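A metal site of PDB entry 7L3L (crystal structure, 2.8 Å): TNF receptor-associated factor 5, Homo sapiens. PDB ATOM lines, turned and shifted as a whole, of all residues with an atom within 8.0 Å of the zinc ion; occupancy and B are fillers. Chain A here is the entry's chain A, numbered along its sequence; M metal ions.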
ATOM      1  N   TYR A  87      -1.661 -23.571  21.092  1.00  0.00           N
ATOM      2  CA  TYR A  87      -1.188 -22.249  20.706  1.00  0.00           C
ATOM      3  C   TYR A  87      -1.771 -21.191  21.643  1.00  0.00           C
ATOM      4  O   TYR A  87      -2.817 -21.374  22.270  1.00  0.00           O
ATOM      5  CB  TYR A  87      -1.579 -21.939  19.263  1.00  0.00           C
ATOM      6  CG  TYR A  87      -0.938 -22.861  18.252  1.00  0.00           C
ATOM      7  CD1 TYR A  87       0.440 -22.938  18.140  1.00  0.00           C
ATOM      8  CD2 TYR A  87      -1.713 -23.645  17.412  1.00  0.00           C
ATOM      9  CE1 TYR A  87       1.042 -23.775  17.220  1.00  0.00           C
ATOM     10  CE2 TYR A  87      -1.124 -24.490  16.476  1.00  0.00           C
ATOM     11  CZ  TYR A  87       0.252 -24.552  16.395  1.00  0.00           C
ATOM     12  OH  TYR A  87       0.848 -25.388  15.469  1.00  0.00           O
ATOM     13  N   CYS A  88      -1.063 -20.063  21.736  1.00  0.00           N
ATOM     14  CA  CYS A  88      -1.433 -19.015  22.681  1.00  0.00           C
ATOM     15  C   CYS A  88      -2.653 -18.242  22.197  1.00  0.00           C
ATOM     16  O   CYS A  88      -2.934 -18.156  21.000  1.00  0.00           O
ATOM     17  CB  CYS A  88      -0.278 -18.047  22.909  1.00  0.00           C
ATOM     18  SG  CYS A  88      -0.783 -16.602  23.839  1.00  0.00           S
ATOM     19  N   SER A  89      -3.376 -17.667  23.158  1.00  0.00           N
ATOM     20  CA  SER A  89      -4.597 -16.937  22.861  1.00  0.00           C
ATOM     21  C   SER A  89      -4.342 -15.635  22.109  1.00  0.00           C
ATOM     22  O   SER A  89      -5.281 -15.077  21.535  1.00  0.00           O
ATOM     23  CB  SER A  89      -5.362 -16.646  24.158  1.00  0.00           C
ATOM     24  OG  SER A  89      -6.049 -15.411  24.080  1.00  0.00           O
ATOM     25  N   ASN A  90      -3.112 -15.136  22.121  1.00  0.00           N
ATOM     26  CA  ASN A  90      -2.761 -13.878  21.452  1.00  0.00           C
ATOM     27  C   ASN A  90      -2.463 -14.103  19.981  1.00  0.00           C
ATOM     28  O   ASN A  90      -1.402 -13.730  19.482  1.00  0.00           O
ATOM     29  CB  ASN A  90      -1.562 -13.246  22.147  1.00  0.00           C
ATOM     30  CG  ASN A  90      -1.913 -12.708  23.513  1.00  0.00           C
ATOM     31  OD1 ASN A  90      -2.892 -11.983  23.664  1.00  0.00           O
ATOM     32  ND2 ASN A  90      -1.121 -13.069  24.519  1.00  0.00           N
ATOM     33  N   ALA A  91      -3.448 -14.656  19.252  1.00  0.00           N
ATOM     34  CA  ALA A  91      -3.189 -15.673  18.236  1.00  0.00           C
ATOM     35  C   ALA A  91      -1.949 -15.428  17.384  1.00  0.00           C
ATOM     36  O   ALA A  91      -1.009 -16.217  17.479  1.00  0.00           O
ATOM     37  CB  ALA A  91      -4.438 -15.857  17.359  1.00  0.00           C
ATOM     38  N   GLY A  93       0.421 -12.734  17.221  1.00  0.00           N
ATOM     39  CA  GLY A  93       1.553 -12.081  17.845  1.00  0.00           C
ATOM     40  C   GLY A  93       2.450 -13.036  18.599  1.00  0.00           C
ATOM     41  O   GLY A  93       3.645 -13.135  18.310  1.00  0.00           O
ATOM     42  N   CYS A  94       1.878 -13.742  19.578  1.00  0.00           N
ATOM     43  CA  CYS A  94       2.666 -14.643  20.416  1.00  0.00           C
ATOM     44  C   CYS A  94       2.899 -15.955  19.692  1.00  0.00           C
ATOM     45  O   CYS A  94       1.969 -16.560  19.150  1.00  0.00           O
ATOM     46  CB  CYS A  94       1.950 -14.894  21.742  1.00  0.00           C
ATOM     47  SG  CYS A  94       2.901 -15.888  22.895  1.00  0.00           S
ATOM     48  N   ASN A  95       4.154 -16.398  19.690  1.00  0.00           N
ATOM     49  CA  ASN A  95       4.546 -17.642  19.049  1.00  0.00           C
ATOM     50  C   ASN A  95       4.677 -18.798  20.029  1.00  0.00           C
ATOM     51  O   ASN A  95       5.220 -19.855  19.665  1.00  0.00           O
ATOM     52  CB  ASN A  95       5.867 -17.444  18.293  1.00  0.00           C
ATOM     53  CG  ASN A  95       5.872 -18.129  16.936  1.00  0.00           C
ATOM     54  OD1 ASN A  95       5.038 -17.846  16.080  1.00  0.00           O
ATOM     55  ND2 ASN A  95       6.831 -19.040  16.745  1.00  0.00           N
ATOM     56  N   ALA A  96       4.198 -18.643  21.258  1.00  0.00           N
ATOM     57  CA  ALA A  96       4.453 -19.616  22.304  1.00  0.00           C
ATOM     58  C   ALA A  96       3.564 -20.839  22.158  1.00  0.00           C
ATOM     59  O   ALA A  96       2.347 -20.718  21.976  1.00  0.00           O
ATOM     60  CB  ALA A  96       4.235 -18.988  23.685  1.00  0.00           C
ATOM     61  N   LYS A  97       4.173 -22.021  22.221  1.00  0.00           N
ATOM     62  CA  LYS A  97       3.465 -23.296  22.325  1.00  0.00           C
ATOM     63  C   LYS A  97       3.537 -23.734  23.781  1.00  0.00           C
ATOM     64  O   LYS A  97       4.573 -24.229  24.235  1.00  0.00           O
ATOM     65  CB  LYS A  97       4.082 -24.345  21.398  1.00  0.00           C
ATOM     66  CG  LYS A  97       3.955 -24.065  19.911  1.00  0.00           C
ATOM     67  CD  LYS A  97       4.616 -25.186  19.109  1.00  0.00           C
ATOM     68  CE  LYS A  97       4.398 -25.005  17.608  1.00  0.00           C
ATOM     69  NZ  LYS A  97       5.059 -26.087  16.813  1.00  0.00           N
ATOM     70  N   VAL A  98       2.450 -23.548  24.507  1.00  0.00           N
ATOM     71  CA  VAL A  98       2.403 -23.840  25.934  1.00  0.00           C
ATOM     72  C   VAL A  98       1.662 -25.155  26.145  1.00  0.00           C
ATOM     73  O   VAL A  98       0.901 -25.622  25.290  1.00  0.00           O
ATOM     74  CB  VAL A  98       1.735 -22.696  26.718  1.00  0.00           C
ATOM     75  CG1 VAL A  98       2.492 -21.399  26.491  1.00  0.00           C
ATOM     76  CG2 VAL A  98       0.288 -22.534  26.289  1.00  0.00           C
ATOM     77  N   TYR A 103      -1.593 -23.217  30.694  1.00  0.00           N
ATOM     78  CA  TYR A 103      -2.065 -22.215  29.758  1.00  0.00           C
ATOM     79  C   TYR A 103      -2.419 -20.914  30.482  1.00  0.00           C
ATOM     80  O   TYR A 103      -2.021 -19.828  30.044  1.00  0.00           O
ATOM     81  CB  TYR A 103      -3.283 -22.764  28.998  1.00  0.00           C
ATOM     82  CG  TYR A 103      -4.064 -21.764  28.170  1.00  0.00           C
ATOM     83  CD1 TYR A 103      -5.040 -20.962  28.744  1.00  0.00           C
ATOM     84  CD2 TYR A 103      -3.842 -21.643  26.800  1.00  0.00           C
ATOM     85  CE1 TYR A 103      -5.760 -20.056  27.996  1.00  0.00           C
ATOM     86  CE2 TYR A 103      -4.561 -20.735  26.038  1.00  0.00           C
ATOM     87  CZ  TYR A 103      -5.518 -19.948  26.645  1.00  0.00           C
ATOM     88  OH  TYR A 103      -6.252 -19.052  25.895  1.00  0.00           O
ATOM     89  N   HIS A 106       0.601 -18.903  31.527  1.00  0.00           N
ATOM     90  CA  HIS A 106       1.338 -18.222  30.472  1.00  0.00           C
ATOM     91  C   HIS A 106       0.751 -16.840  30.201  1.00  0.00           C
ATOM     92  O   HIS A 106       1.491 -15.871  30.045  1.00  0.00           O
ATOM     93  CB  HIS A 106       1.354 -19.043  29.193  1.00  0.00           C
ATOM     94  CG  HIS A 106       1.738 -18.256  27.975  1.00  0.00           C
ATOM     95  ND1 HIS A 106       3.043 -17.882  27.716  1.00  0.00           N
ATOM     96  CD2 HIS A 106       0.995 -17.761  26.960  1.00  0.00           C
ATOM     97  CE1 HIS A 106       3.076 -17.186  26.590  1.00  0.00           C
ATOM     98  NE2 HIS A 106       1.851 -17.104  26.106  1.00  0.00           N
ATOM     99  N   LEU A 107      -0.582 -16.757  30.108  1.00  0.00           N
ATOM    100  CA  LEU A 107      -1.219 -15.468  29.841  1.00  0.00           C
ATOM    101  C   LEU A 107      -0.908 -14.446  30.918  1.00  0.00           C
ATOM    102  O   LEU A 107      -0.857 -13.249  30.643  1.00  0.00           O
ATOM    103  CB  LEU A 107      -2.727 -15.652  29.700  1.00  0.00           C
ATOM    104  CG  LEU A 107      -3.213 -16.749  28.746  1.00  0.00           C
ATOM    105  CD1 LEU A 107      -4.702 -16.606  28.477  1.00  0.00           C
ATOM    106  CD2 LEU A 107      -2.427 -16.727  27.454  1.00  0.00           C
ATOM    107  N   GLN A 108      -0.685 -14.906  32.162  1.00  0.00           N
ATOM    108  CA  GLN A 108      -0.331 -13.994  33.236  1.00  0.00           C
ATOM    109  C   GLN A 108       1.028 -13.342  33.015  1.00  0.00           C
ATOM    110  O   GLN A 108       1.336 -12.348  33.678  1.00  0.00           O
ATOM    111  CB  GLN A 108      -0.338 -14.738  34.578  1.00  0.00           C
ATOM    112  CG  GLN A 108      -1.719 -15.248  34.968  1.00  0.00           C
ATOM    113  CD  GLN A 108      -2.813 -14.249  34.651  1.00  0.00           C
ATOM    114  OE1 GLN A 108      -3.704 -14.522  33.839  1.00  0.00           O
ATOM    115  NE2 GLN A 108      -2.759 -13.079  35.276  1.00  0.00           N
ATOM    116  N   GLN A 109       1.841 -13.873  32.101  1.00  0.00           N
ATOM    117  CA  GLN A 109       3.142 -13.286  31.786  1.00  0.00           C
ATOM    118  C   GLN A 109       3.326 -13.002  30.299  1.00  0.00           C
ATOM    119  O   GLN A 109       4.339 -12.407  29.923  1.00  0.00           O
ATOM    120  CB  GLN A 109       4.277 -14.211  32.269  1.00  0.00           C
ATOM    121  CG  GLN A 109       4.387 -15.502  31.471  1.00  0.00           C
ATOM    122  CD  GLN A 109       5.781 -16.102  31.504  1.00  0.00           C
ATOM    123  OE1 GLN A 109       6.100 -17.022  30.752  1.00  0.00           O
ATOM    124  NE2 GLN A 109       6.634 -15.564  32.369  1.00  0.00           N
ATOM    125  N   CYS A 110       2.373 -13.392  29.456  1.00  0.00           N
ATOM    126  CA  CYS A 110       2.577 -13.309  28.014  1.00  0.00           C
ATOM    127  C   CYS A 110       2.565 -11.857  27.550  1.00  0.00           C
ATOM    128  O   CYS A 110       1.663 -11.095  27.897  1.00  0.00           O
ATOM    129  CB  CYS A 110       1.486 -14.075  27.278  1.00  0.00           C
ATOM    130  SG  CYS A 110       1.670 -13.964  25.502  1.00  0.00           S
ATOM    131  N   LEU A 111       3.562 -11.500  26.736  1.00  0.00           N
ATOM    132  CA  LEU A 111       3.780 -10.110  26.351  1.00  0.00           C
ATOM    133  C   LEU A 111       2.554  -9.500  25.694  1.00  0.00           C
ATOM    134  O   LEU A 111       2.236  -8.325  25.924  1.00  0.00           O
ATOM    135  CB  LEU A 111       4.947 -10.007  25.378  1.00  0.00           C
ATOM    136  CG  LEU A 111       6.257 -10.732  25.594  1.00  0.00           C
ATOM    137  CD1 LEU A 111       7.165 -10.542  24.395  1.00  0.00           C
ATOM    138  CD2 LEU A 111       6.916 -10.171  26.835  1.00  0.00           C
ATOM    139  N   PHE A 112       1.856 -10.276  24.866  1.00  0.00           N
ATOM    140  CA  PHE A 112       0.912  -9.702  23.914  1.00  0.00           C
ATOM    141  C   PHE A 112      -0.531  -9.811  24.386  1.00  0.00           C
ATOM    142  O   PHE A 112      -1.454  -9.493  23.618  1.00  0.00           O
ATOM    143  CB  PHE A 112       1.073 -10.375  22.551  1.00  0.00           C
ATOM    144  CG  PHE A 112       2.471 -10.270  21.983  1.00  0.00           C
ATOM    145  CD1 PHE A 112       3.406  -9.412  22.534  1.00  0.00           C
ATOM    146  CD2 PHE A 112       2.853 -11.029  20.896  1.00  0.00           C
ATOM    147  CE1 PHE A 112       4.689  -9.338  22.013  1.00  0.00           C
ATOM    148  CE2 PHE A 112       4.129 -10.943  20.370  1.00  0.00           C
ATOM    149  CZ  PHE A 112       5.050 -10.098  20.932  1.00  0.00           C
ATOM    150  N   GLN A 113      -0.760 -10.223  25.618  1.00  0.00           N
ATOM    151  CA  GLN A 113      -2.127 -10.194  26.125  1.00  0.00           C
ATOM    152  C   GLN A 113      -2.433  -8.827  26.705  1.00  0.00           C
ATOM    153  O   GLN A 113      -1.648  -8.310  27.505  1.00  0.00           O
ATOM    154  CB  GLN A 113      -2.346 -11.274  27.168  1.00  0.00           C
ATOM    155  CG  GLN A 113      -3.730 -11.881  27.131  1.00  0.00           C
ATOM    156  CD  GLN A 113      -4.543 -11.549  28.369  1.00  0.00           C
ATOM    157  OE1 GLN A 113      -4.033 -10.936  29.304  1.00  0.00           O
ATOM    158  NE2 GLN A 113      -5.809 -11.960  28.378  1.00  0.00           N
ATOM    159  N   ARG A 128       0.996  -5.982  27.246  1.00  0.00           N
ATOM    160  CA  ARG A 128       1.909  -6.091  28.387  1.00  0.00           C
ATOM    161  C   ARG A 128       3.304  -5.594  28.011  1.00  0.00           C
ATOM    162  O   ARG A 128       3.968  -4.925  28.811  1.00  0.00           O
ATOM    163  CB  ARG A 128       1.970  -7.537  28.875  1.00  0.00           C
ATOM    164  CG  ARG A 128       2.771  -7.692  30.155  1.00  0.00           C
ATOM    165  CD  ARG A 128       2.688  -9.119  30.697  1.00  0.00           C
ATOM    166  NE  ARG A 128       1.553  -9.298  31.587  1.00  0.00           N
ATOM    167  CZ  ARG A 128       0.540 -10.129  31.346  1.00  0.00           C
ATOM    168  NH1 ARG A 128       0.512 -10.848  30.234  1.00  0.00           N
ATOM    169  NH2 ARG A 128      -0.447 -10.232  32.220  1.00  0.00           N
HETATM  170 ZN    ZN M   1       1.103 -15.816  24.511  1.00  0.00          ZN
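N of Asn 90 sits close to SG of Cys 88.
The backbone carbonyl oxygen (O) of Ala 96 sits at hydrogen-bond distance from the backbone NH (N) of Cys 88.
SG of Cys 110 lies close to ND2 of Asn 90, 3.1 Å away.
The side-chain sulfur (SG) of Cys 110 sits close to the backbone NH (N) of Phe 112 (3.7 Å).
NH1 of Arg 128 is in hydrogen-bond range of O of Cys 110, at 2.6 Å.
N of Ala 96 sits close to SG of Cys 94, 3.5 Å away.
OD1 of Asn 90 lies close to O of Phe 112, 2.9 Å away.
ND2 of Asn 90 lies close to N of Gln 113, 3.1 Å away.
Asn 90 touches the zinc ion.
Within 4 Å of the zinc ion: Cys 88, Asn 90, Cys 94, His 106 and Cys 110.
The nearest printed residue that does not touch the zinc ion is Ala 96 (4.5 Å).
The zinc ion is bound by the side-chain sulfur (SG) of Cys 88 (2.2 Å).
The zinc ion is bound by SG of Cys 110, at 2.2 Å.
The zinc ion is bound by NE2 of His 106, at 2.2 Å.
SG of Cys 94 binds the zinc ion, 2.4 Å away.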
